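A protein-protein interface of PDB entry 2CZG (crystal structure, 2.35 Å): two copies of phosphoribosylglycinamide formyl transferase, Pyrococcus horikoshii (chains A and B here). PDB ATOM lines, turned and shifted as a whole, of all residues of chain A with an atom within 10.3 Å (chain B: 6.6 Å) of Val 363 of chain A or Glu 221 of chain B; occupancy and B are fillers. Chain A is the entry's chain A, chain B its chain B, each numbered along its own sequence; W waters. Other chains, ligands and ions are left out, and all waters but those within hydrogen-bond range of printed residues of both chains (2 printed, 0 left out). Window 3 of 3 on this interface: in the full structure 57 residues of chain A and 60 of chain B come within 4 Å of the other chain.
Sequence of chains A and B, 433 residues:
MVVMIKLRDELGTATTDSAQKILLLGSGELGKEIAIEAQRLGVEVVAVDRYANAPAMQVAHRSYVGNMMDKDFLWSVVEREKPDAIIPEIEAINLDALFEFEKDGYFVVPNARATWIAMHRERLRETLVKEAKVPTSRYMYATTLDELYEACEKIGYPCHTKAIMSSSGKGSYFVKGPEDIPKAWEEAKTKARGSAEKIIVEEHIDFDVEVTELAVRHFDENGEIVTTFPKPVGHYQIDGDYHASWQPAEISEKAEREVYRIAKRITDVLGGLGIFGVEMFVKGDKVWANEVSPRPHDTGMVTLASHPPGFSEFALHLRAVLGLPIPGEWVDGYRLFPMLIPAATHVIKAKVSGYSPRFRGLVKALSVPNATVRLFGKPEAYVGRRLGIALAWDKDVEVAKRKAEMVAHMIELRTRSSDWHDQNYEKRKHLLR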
ATOM      1  N   PHE A 359     -23.143  14.499  31.397  1.00  0.00           N
ATOM      2  CA  PHE A 359     -21.963  13.716  31.047  1.00  0.00           C
ATOM      3  C   PHE A 359     -20.675  14.471  31.377  1.00  0.00           C
ATOM      4  O   PHE A 359     -20.606  15.690  31.192  1.00  0.00           O
ATOM      5  CB  PHE A 359     -21.994  13.404  29.530  1.00  0.00           C
ATOM      6  CG  PHE A 359     -23.365  13.000  29.008  1.00  0.00           C
ATOM      7  CD1 PHE A 359     -24.379  13.947  28.866  1.00  0.00           C
ATOM      8  CD2 PHE A 359     -23.659  11.667  28.728  1.00  0.00           C
ATOM      9  CE1 PHE A 359     -25.665  13.574  28.463  1.00  0.00           C
ATOM     10  CE2 PHE A 359     -24.955  11.271  28.321  1.00  0.00           C
ATOM     11  CZ  PHE A 359     -25.955  12.225  28.189  1.00  0.00           C
ATOM     12  N   ARG A 360     -19.661  13.750  31.865  1.00  0.00           N
ATOM     13  CA  ARG A 360     -18.359  14.348  32.193  1.00  0.00           C
ATOM     14  C   ARG A 360     -17.249  13.514  31.547  1.00  0.00           C
ATOM     15  O   ARG A 360     -17.502  12.433  31.015  1.00  0.00           O
ATOM     16  CB  ARG A 360     -18.124  14.397  33.705  1.00  0.00           C
ATOM     17  CG  ARG A 360     -18.204  13.024  34.335  1.00  0.00           C
ATOM     18  CD  ARG A 360     -17.308  12.842  35.540  1.00  0.00           C
ATOM     19  NE  ARG A 360     -17.574  13.778  36.622  1.00  0.00           N
ATOM     20  CZ  ARG A 360     -17.463  13.455  37.907  1.00  0.00           C
ATOM     21  NH1 ARG A 360     -17.106  12.219  38.249  1.00  0.00           N
ATOM     22  NH2 ARG A 360     -17.683  14.366  38.848  1.00  0.00           N
ATOM     23  N   GLY A 361     -16.018  14.018  31.607  1.00  0.00           N
ATOM     24  CA  GLY A 361     -14.897  13.316  31.010  1.00  0.00           C
ATOM     25  C   GLY A 361     -14.742  13.755  29.566  1.00  0.00           C
ATOM     26  O   GLY A 361     -14.060  13.106  28.770  1.00  0.00           O
ATOM     27  N   LEU A 362     -15.374  14.875  29.228  1.00  0.00           N
ATOM     28  CA  LEU A 362     -15.324  15.385  27.861  1.00  0.00           C
ATOM     29  C   LEU A 362     -13.976  15.994  27.492  1.00  0.00           C
ATOM     30  O   LEU A 362     -13.582  15.971  26.324  1.00  0.00           O
ATOM     31  CB  LEU A 362     -16.466  16.392  27.632  1.00  0.00           C
ATOM     32  CG  LEU A 362     -17.886  15.822  27.831  1.00  0.00           C
ATOM     33  CD1 LEU A 362     -18.931  16.906  27.614  1.00  0.00           C
ATOM     34  CD2 LEU A 362     -18.113  14.670  26.863  1.00  0.00           C
ATOM     35  N   VAL A 363     -13.254  16.526  28.472  1.00  0.00           N
ATOM     36  CA  VAL A 363     -11.940  17.103  28.183  1.00  0.00           C
ATOM     37  C   VAL A 363     -11.043  16.046  27.529  1.00  0.00           C
ATOM     38  O   VAL A 363     -10.350  16.325  26.534  1.00  0.00           O
ATOM     39  CB  VAL A 363     -11.233  17.606  29.459  1.00  0.00           C
ATOM     40  CG1 VAL A 363      -9.757  17.896  29.145  1.00  0.00           C
ATOM     41  CG2 VAL A 363     -11.938  18.860  29.999  1.00  0.00           C
ATOM     42  N   LYS A 364     -11.050  14.836  28.085  1.00  0.00           N
ATOM     43  CA  LYS A 364     -10.223  13.756  27.531  1.00  0.00           C
ATOM     44  C   LYS A 364     -10.925  13.057  26.373  1.00  0.00           C
ATOM     45  O   LYS A 364     -10.303  12.733  25.367  1.00  0.00           O
ATOM     46  CB  LYS A 364      -9.870  12.725  28.618  1.00  0.00           C
ATOM     47  CG  LYS A 364      -9.174  13.326  29.830  1.00  0.00           C
ATOM     48  CD  LYS A 364      -8.006  12.477  30.328  1.00  0.00           C
ATOM     49  CE  LYS A 364      -8.443  11.108  30.815  1.00  0.00           C
ATOM     50  NZ  LYS A 364      -7.276  10.250  31.199  1.00  0.00           N
ATOM     51  N   ALA A 365     -12.224  12.829  26.509  1.00  0.00           N
ATOM     52  CA  ALA A 365     -12.983  12.171  25.450  1.00  0.00           C
ATOM     53  C   ALA A 365     -13.001  12.944  24.144  1.00  0.00           C
ATOM     54  O   ALA A 365     -12.898  12.349  23.070  1.00  0.00           O
ATOM     55  CB  ALA A 365     -14.396  11.931  25.901  1.00  0.00           C
ATOM     56  N   LEU A 366     -13.121  14.270  24.233  1.00  0.00           N
ATOM     57  CA  LEU A 366     -13.194  15.112  23.042  1.00  0.00           C
ATOM     58  C   LEU A 366     -11.853  15.627  22.541  1.00  0.00           C
ATOM     59  O   LEU A 366     -11.804  16.403  21.590  1.00  0.00           O
ATOM     60  CB  LEU A 366     -14.166  16.289  23.268  1.00  0.00           C
ATOM     61  CG  LEU A 366     -15.600  15.911  23.686  1.00  0.00           C
ATOM     62  CD1 LEU A 366     -16.487  17.151  23.767  1.00  0.00           C
ATOM     63  CD2 LEU A 366     -16.171  14.912  22.687  1.00  0.00           C
ATOM     64  N   SER A 367     -10.763  15.204  23.171  1.00  0.00           N
ATOM     65  CA  SER A 367      -9.435  15.611  22.712  1.00  0.00           C
ATOM     66  C   SER A 367      -8.851  14.517  21.813  1.00  0.00           C
ATOM     67  O   SER A 367      -7.825  14.713  21.175  1.00  0.00           O
ATOM     68  CB  SER A 367      -8.504  15.863  23.892  1.00  0.00           C
ATOM     69  OG  SER A 367      -8.876  17.041  24.594  1.00  0.00           O
ATOM     70  N   VAL A 368      -9.521  13.367  21.760  1.00  0.00           N
ATOM     71  CA  VAL A 368      -9.067  12.257  20.934  1.00  0.00           C
ATOM     72  C   VAL A 368      -9.254  12.585  19.446  1.00  0.00           C
ATOM     73  O   VAL A 368     -10.353  12.913  18.997  1.00  0.00           O
ATOM     74  CB  VAL A 368      -9.851  10.964  21.278  1.00  0.00           C
ATOM     75  CG1 VAL A 368      -9.399   9.830  20.379  1.00  0.00           C
ATOM     76  CG2 VAL A 368      -9.651  10.607  22.761  1.00  0.00           C
ATOM     77  N   PRO A 369      -8.174  12.509  18.661  1.00  0.00           N
ATOM     78  CA  PRO A 369      -8.244  12.802  17.223  1.00  0.00           C
ATOM     79  C   PRO A 369      -9.153  11.865  16.430  1.00  0.00           C
ATOM     80  O   PRO A 369      -9.299  10.689  16.771  1.00  0.00           O
ATOM     81  CB  PRO A 369      -6.783  12.673  16.763  1.00  0.00           C
ATOM     82  CG  PRO A 369      -5.999  13.016  18.003  1.00  0.00           C
ATOM     83  CD  PRO A 369      -6.773  12.331  19.106  1.00  0.00           C
ATOM     84  N   VAL A 373     -18.502  12.695  19.713  1.00  0.00           N
ATOM     85  CA  VAL A 373     -19.630  12.003  20.295  1.00  0.00           C
ATOM     86  C   VAL A 373     -20.923  12.665  19.842  1.00  0.00           C
ATOM     87  O   VAL A 373     -20.904  13.743  19.259  1.00  0.00           O
ATOM     88  CB  VAL A 373     -19.567  12.033  21.832  1.00  0.00           C
ATOM     89  CG1 VAL A 373     -18.228  11.499  22.294  1.00  0.00           C
ATOM     90  CG2 VAL A 373     -19.794  13.451  22.347  1.00  0.00           C
ATOM     91  N   MET A 406     -12.675   3.586  23.146  1.00  0.00           N
ATOM     92  CA  MET A 406     -11.930   4.374  24.115  1.00  0.00           C
ATOM     93  C   MET A 406     -12.624   5.708  24.430  1.00  0.00           C
ATOM     94  O   MET A 406     -12.655   6.133  25.584  1.00  0.00           O
ATOM     95  CB  MET A 406     -10.492   4.609  23.613  1.00  0.00           C
ATOM     96  CG  MET A 406      -9.650   5.481  24.534  1.00  0.00           C
ATOM     97  SD  MET A 406      -7.929   5.711  23.975  1.00  0.00           S
ATOM     98  CE  MET A 406      -8.108   7.018  22.744  1.00  0.00           C
ATOM     99  N   VAL A 407     -13.186   6.366  23.417  1.00  0.00           N
ATOM    100  CA  VAL A 407     -13.880   7.639  23.645  1.00  0.00           C
ATOM    101  C   VAL A 407     -15.130   7.420  24.484  1.00  0.00           C
ATOM    102  O   VAL A 407     -15.432   8.193  25.394  1.00  0.00           O
ATOM    103  CB  VAL A 407     -14.291   8.314  22.318  1.00  0.00           C
ATOM    104  CG1 VAL A 407     -15.239   9.492  22.591  1.00  0.00           C
ATOM    105  CG2 VAL A 407     -13.041   8.798  21.588  1.00  0.00           C
ATOM    106  N   MET A 410     -14.312   6.865  28.209  1.00  0.00           N
ATOM    107  CA  MET A 410     -13.773   7.986  28.986  1.00  0.00           C
ATOM    108  C   MET A 410     -14.917   8.837  29.544  1.00  0.00           C
ATOM    109  O   MET A 410     -14.685   9.782  30.284  1.00  0.00           O
ATOM    110  CB  MET A 410     -12.895   8.886  28.114  1.00  0.00           C
ATOM    111  CG  MET A 410     -11.644   8.221  27.544  1.00  0.00           C
ATOM    112  SD  MET A 410     -10.756   9.289  26.371  1.00  0.00           S
ATOM    113  CE  MET A 410      -9.044   8.892  26.772  1.00  0.00           C
ATOM    114  N   ILE A 411     -16.154   8.487  29.203  1.00  0.00           N
ATOM    115  CA  ILE A 411     -17.315   9.259  29.628  1.00  0.00           C
ATOM    116  C   ILE A 411     -18.126   8.705  30.803  1.00  0.00           C
ATOM    117  O   ILE A 411     -18.421   7.517  30.848  1.00  0.00           O
ATOM    118  CB  ILE A 411     -18.241   9.483  28.401  1.00  0.00           C
ATOM    119  CG1 ILE A 411     -17.578  10.489  27.456  1.00  0.00           C
ATOM    120  CG2 ILE A 411     -19.619   9.963  28.835  1.00  0.00           C
ATOM    121  CD1 ILE A 411     -18.132  10.498  26.047  1.00  0.00           C
ATOM    122  N   GLU A 412     -18.486   9.577  31.750  1.00  0.00           N
ATOM    123  CA  GLU A 412     -19.291   9.166  32.912  1.00  0.00           C
ATOM    124  C   GLU A 412     -20.626   9.896  32.881  1.00  0.00           C
ATOM    125  O   GLU A 412     -20.692  11.066  32.496  1.00  0.00           O
ATOM    126  CB  GLU A 412     -18.582   9.477  34.235  1.00  0.00           C
ATOM    127  CG  GLU A 412     -17.163   8.943  34.321  1.00  0.00           C
ATOM    128  CD  GLU A 412     -16.642   8.864  35.748  1.00  0.00           C
ATOM    129  OE1 GLU A 412     -16.803   9.843  36.517  1.00  0.00           O
ATOM    130  OE2 GLU A 412     -16.059   7.814  36.092  1.00  0.00           O
ATOM    131  N   LEU B   7     -12.182  25.847  30.602  1.00  0.00           N
ATOM    132  CA  LEU B   7     -12.170  24.516  29.999  1.00  0.00           C
ATOM    133  C   LEU B   7     -13.421  23.788  30.457  1.00  0.00           C
ATOM    134  O   LEU B   7     -13.727  23.772  31.640  1.00  0.00           O
ATOM    135  CB  LEU B   7     -10.958  23.723  30.485  1.00  0.00           C
ATOM    136  CG  LEU B   7     -10.218  22.793  29.520  1.00  0.00           C
ATOM    137  CD1 LEU B   7      -9.629  21.641  30.343  1.00  0.00           C
ATOM    138  CD2 LEU B   7     -11.133  22.277  28.401  1.00  0.00           C
ATOM    139  N   ARG B   8     -14.132  23.161  29.534  1.00  0.00           N
ATOM    140  CA  ARG B   8     -15.369  22.483  29.898  1.00  0.00           C
ATOM    141  C   ARG B   8     -15.223  20.968  29.825  1.00  0.00           C
ATOM    142  O   ARG B   8     -14.733  20.437  28.828  1.00  0.00           O
ATOM    143  CB  ARG B   8     -16.482  22.987  28.974  1.00  0.00           C
ATOM    144  CG  ARG B   8     -17.806  22.283  29.114  1.00  0.00           C
ATOM    145  CD  ARG B   8     -18.952  23.144  28.568  1.00  0.00           C
ATOM    146  NE  ARG B   8     -20.066  22.904  29.461  1.00  0.00           N
ATOM    147  CZ  ARG B   8     -20.677  23.832  30.170  1.00  0.00           C
ATOM    148  NH1 ARG B   8     -20.316  25.108  30.083  1.00  0.00           N
ATOM    149  NH2 ARG B   8     -21.593  23.450  31.038  1.00  0.00           N
ATOM    150  N   ASP B   9     -15.642  20.280  30.885  1.00  0.00           N
ATOM    151  CA  ASP B   9     -15.535  18.816  30.938  1.00  0.00           C
ATOM    152  C   ASP B   9     -16.904  18.131  31.014  1.00  0.00           C
ATOM    153  O   ASP B   9     -16.998  16.896  30.943  1.00  0.00           O
ATOM    154  CB  ASP B   9     -14.690  18.388  32.165  1.00  0.00           C
ATOM    155  CG  ASP B   9     -14.415  16.869  32.199  1.00  0.00           C
ATOM    156  OD1 ASP B   9     -13.716  16.357  31.288  1.00  0.00           O
ATOM    157  OD2 ASP B   9     -14.902  16.189  33.132  1.00  0.00           O
ATOM    158  N   GLU B  10     -17.963  18.925  31.139  1.00  0.00           N
ATOM    159  CA  GLU B  10     -19.292  18.354  31.283  1.00  0.00           C
ATOM    160  C   GLU B  10     -20.390  19.023  30.458  1.00  0.00           C
ATOM    161  O   GLU B  10     -20.301  20.193  30.109  1.00  0.00           O
ATOM    162  CB  GLU B  10     -19.661  18.373  32.776  1.00  0.00           C
ATOM    163  CG  GLU B  10     -21.062  17.893  33.155  1.00  0.00           C
ATOM    164  CD  GLU B  10     -22.120  18.994  33.109  1.00  0.00           C
ATOM    165  OE1 GLU B  10     -21.754  20.180  32.940  1.00  0.00           O
ATOM    166  OE2 GLU B  10     -23.326  18.671  33.251  1.00  0.00           O
ATOM    167  N   PHE B 219     -10.003  26.177  23.948  1.00  0.00           N
ATOM    168  CA  PHE B 219      -9.176  25.654  25.029  1.00  0.00           C
ATOM    169  C   PHE B 219      -8.509  24.343  24.632  1.00  0.00           C
ATOM    170  O   PHE B 219      -9.072  23.562  23.864  1.00  0.00           O
ATOM    171  CB  PHE B 219     -10.030  25.411  26.276  1.00  0.00           C
ATOM    172  CG  PHE B 219     -10.387  26.664  27.028  1.00  0.00           C
ATOM    173  CD1 PHE B 219      -9.390  27.460  27.592  1.00  0.00           C
ATOM    174  CD2 PHE B 219     -11.715  27.020  27.220  1.00  0.00           C
ATOM    175  CE1 PHE B 219      -9.714  28.598  28.347  1.00  0.00           C
ATOM    176  CE2 PHE B 219     -12.055  28.151  27.970  1.00  0.00           C
ATOM    177  CZ  PHE B 219     -11.046  28.945  28.539  1.00  0.00           C
ATOM    178  N   ASP B 220      -7.294  24.108  25.131  1.00  0.00           N
ATOM    179  CA  ASP B 220      -6.630  22.850  24.849  1.00  0.00           C
ATOM    180  C   ASP B 220      -6.849  21.982  26.070  1.00  0.00           C
ATOM    181  O   ASP B 220      -7.477  22.422  27.040  1.00  0.00           O
ATOM    182  CB  ASP B 220      -5.127  23.027  24.562  1.00  0.00           C
ATOM    183  CG  ASP B 220      -4.338  23.549  25.754  1.00  0.00           C
ATOM    184  OD1 ASP B 220      -4.840  23.541  26.904  1.00  0.00           O
ATOM    185  OD2 ASP B 220      -3.183  23.965  25.524  1.00  0.00           O
ATOM    186  N   GLU B 221      -6.339  20.755  26.032  1.00  0.00           N
ATOM    187  CA  GLU B 221      -6.499  19.816  27.140  1.00  0.00           C
ATOM    188  C   GLU B 221      -6.023  20.393  28.473  1.00  0.00           C
ATOM    189  O   GLU B 221      -6.504  19.993  29.526  1.00  0.00           O
ATOM    190  CB  GLU B 221      -5.731  18.526  26.825  1.00  0.00           C
ATOM    191  CG  GLU B 221      -6.274  17.274  27.507  1.00  0.00           C
ATOM    192  CD  GLU B 221      -5.886  15.983  26.776  1.00  0.00           C
ATOM    193  OE1 GLU B 221      -6.388  14.905  27.162  1.00  0.00           O
ATOM    194  OE2 GLU B 221      -5.083  16.044  25.815  1.00  0.00           O
ATOM    195  N   ASN B 222      -5.095  21.343  28.440  1.00  0.00           N
ATOM    196  CA  ASN B 222      -4.578  21.908  29.689  1.00  0.00           C
ATOM    197  C   ASN B 222      -5.345  23.100  30.224  1.00  0.00           C
ATOM    198  O   ASN B 222      -4.965  23.669  31.245  1.00  0.00           O
ATOM    199  CB  ASN B 222      -3.104  22.310  29.545  1.00  0.00           C
ATOM    200  CG  ASN B 222      -2.173  21.112  29.419  1.00  0.00           C
ATOM    201  OD1 ASN B 222      -0.989  21.272  29.126  1.00  0.00           O
ATOM    202  ND2 ASN B 222      -2.699  19.912  29.646  1.00  0.00           N
ATOM    203  N   GLY B 223      -6.419  23.483  29.544  1.00  0.00           N
ATOM    204  CA  GLY B 223      -7.194  24.621  30.009  1.00  0.00           C
ATOM    205  C   GLY B 223      -6.645  25.939  29.488  1.00  0.00           C
ATOM    206  O   GLY B 223      -7.042  27.012  29.933  1.00  0.00           O
ATOM    207  N   GLU B 224      -5.718  25.857  28.545  1.00  0.00           N
ATOM    208  CA  GLU B 224      -5.141  27.057  27.963  1.00  0.00           C
ATOM    209  C   GLU B 224      -5.634  27.270  26.539  1.00  0.00           C
ATOM    210  O   GLU B 224      -5.978  26.334  25.826  1.00  0.00           O
ATOM    211  CB  GLU B 224      -3.617  26.979  28.000  1.00  0.00           C
ATOM    212  CG  GLU B 224      -3.093  26.926  29.424  1.00  0.00           C
ATOM    213  CD  GLU B 224      -1.595  27.024  29.497  1.00  0.00           C
ATOM    214  OE1 GLU B 224      -0.908  26.124  28.966  1.00  0.00           O
ATOM    215  OE2 GLU B 224      -1.107  28.009  30.084  1.00  0.00           O
ATOM    216  N   GLY B 323     -16.344  26.065  25.430  1.00  0.00           N
ATOM    217  CA  GLY B 323     -15.158  25.765  26.221  1.00  0.00           C
ATOM    218  C   GLY B 323     -14.664  24.327  26.087  1.00  0.00           C
ATOM    219  O   GLY B 323     -13.868  23.848  26.908  1.00  0.00           O
ATOM    220  N   LEU B 324     -15.142  23.633  25.056  1.00  0.00           N
ATOM    221  CA  LEU B 324     -14.765  22.237  24.815  1.00  0.00           C
ATOM    222  C   LEU B 324     -13.526  22.184  23.946  1.00  0.00           C
ATOM    223  O   LEU B 324     -13.263  23.102  23.169  1.00  0.00           O
ATOM    224  CB  LEU B 324     -15.903  21.487  24.094  1.00  0.00           C
ATOM    225  CG  LEU B 324     -17.204  21.242  24.859  1.00  0.00           C
ATOM    226  CD1 LEU B 324     -18.289  20.880  23.880  1.00  0.00           C
ATOM    227  CD2 LEU B 324     -17.025  20.134  25.901  1.00  0.00           C
ATOM    228  N   PRO B 325     -12.743  21.103  24.059  1.00  0.00           N
ATOM    229  CA  PRO B 325     -11.530  20.973  23.250  1.00  0.00           C
ATOM    230  C   PRO B 325     -11.813  20.660  21.794  1.00  0.00           C
ATOM    231  O   PRO B 325     -12.934  20.320  21.422  1.00  0.00           O
ATOM    232  CB  PRO B 325     -10.775  19.834  23.931  1.00  0.00           C
ATOM    233  CG  PRO B 325     -11.855  18.988  24.469  1.00  0.00           C
ATOM    234  CD  PRO B 325     -12.843  20.003  25.031  1.00  0.00           C
ATOM    235  N   ARG B 335      -0.581  24.506  15.038  1.00  0.00           N
ATOM    236  CA  ARG B 335      -1.578  23.499  15.402  1.00  0.00           C
ATOM    237  C   ARG B 335      -2.640  23.519  14.312  1.00  0.00           C
ATOM    238  O   ARG B 335      -3.520  24.384  14.302  1.00  0.00           O
ATOM    239  CB  ARG B 335      -2.221  23.826  16.749  1.00  0.00           C
ATOM    240  CG  ARG B 335      -3.063  22.688  17.333  1.00  0.00           C
ATOM    241  CD  ARG B 335      -3.493  23.054  18.729  1.00  0.00           C
ATOM    242  NE  ARG B 335      -4.089  21.957  19.484  1.00  0.00           N
ATOM    243  CZ  ARG B 335      -5.248  21.366  19.198  1.00  0.00           C
ATOM    244  NH1 ARG B 335      -5.970  21.742  18.146  1.00  0.00           N
ATOM    245  NH2 ARG B 335      -5.711  20.426  20.007  1.00  0.00           N
HETATM  246  O   HOH W   1     -11.786  14.524  31.038  1.00  0.00           O
HETATM  247  O   HOH W   2      -7.357  18.969  23.253  1.00  0.00           O
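The side-chain carboxylate of Asp 9 of chain B sits at hydrogen-bond distance from the backbone NH of Gly 361 of chain A (2.9 Å). OD1 of Asp 9 of chain B lies within hydrogen-bond range of N of Leu 362 of chain A (3.0 Å). The backbone NH of Val 363 of chain A is in hydrogen-bond range of the side-chain carboxylate of Asp 9 of chain B, at 2.9 Å.
The guanidinium group of Arg 360 of chain A lies within salt-bridge range of the side-chain carboxylate of Glu 412 of chain A. The side-chain hydroxyl (OG) of Ser 367 of chain A sits at hydrogen-bond distance from the backbone carbonyl oxygen (O) of Val 363 of chain A. NH2 of Arg 8 of chain B is in salt-bridge range of OE1 of Glu 10 of chain B (3.8 Å). O of Gly 323 of chain B is in hydrogen-bond range of N of Arg 8 of chain B (2.7 Å).
O of Asp 9 of chain B touches O of Phe 359 of chain A, 3.8 Å away. O of Phe 359 of chain A touches CA of Glu 10 of chain B, 3.0 Å away. Arg 360 of chain A touches Asp 9 of chain B. Pro 325 of chain B touches Leu 362 of chain A. Leu 7 of chain B touches Val 363 of chain A. O of Arg 8 of chain B touches CG2 of Val 363 of chain A (3.4 Å). O of Glu 221 of chain B touches CG1 of Val 363 of chain A, at 3.9 Å. Val 363 of chain A touches Pro 325 of chain B (O to CG, 3.7 Å). Leu 324 of chain B touches Leu 366 of chain A (CD2 to CD1, 3.7 Å). Pro 325 of chain B touches Ser 367 of chain A.
Of the printed residues of chain B, Arg 360 of chain A touches Asp 9. Of the printed residues of chain B, Gly 361 of chain A touches Asp 9 (2.9 Å). Printed residues of chain B within 4 Å of Leu 362 of chain A: Asp 9 (3.0 Å), Glu 10 (3.8 Å) and Pro 325 (3.9 Å). Val 363 of chain A touches five residues of chain B. Printed residues of chain B within 4 Å of Leu 366 of chain A: Leu 324 and Pro 325. Asp 9 of chain B touches five residues of chain A. No residue of chain A comes within 4 Å of Asp 220 of chain B. Of chain A, only Val 363 and Ser 367 come within 4 Å of Glu 221 of chain B. Asn 222 of chain B touches none of the printed residues of chain A. Glu 224 of chain B touches none of the printed residues of chain A. Of the printed residues of chain A, Pro 325 of chain B touches Leu 362 (3.9 Å), Val 363 (3.7 Å), Leu 366 (3.8 Å) and Ser 367 (3.4 Å). The nearest residue of chain A that does not touch Glu 221 of chain B is Lys 364 of chain A (4.02 Å). The nearest printed residue of chain B that does not touch Phe 359 of chain A is Arg 8 of chain B (7.4 Å).
Hydrophobic or aromatic side chains of chain B that line the printed part of chain A: Leu 7, Leu 324 and Pro 325. Among the printed residues, no Asp or Glu carboxylate lies within 4 Å of a Lys or Arg side-chain nitrogen of the other chain.
No position is printed for both chains.
Water W1 bridges the side-chain carboxylate of Asp 9 of chain B (2.7 Å) and the backbone NH of Lys 364 of chain A (3.1 Å). Water W2 bridges the side-chain hydroxyl of Ser 367 of chain A (2.8 Å) and the backbone NH of Glu 221 of chain B (3.5 Å).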
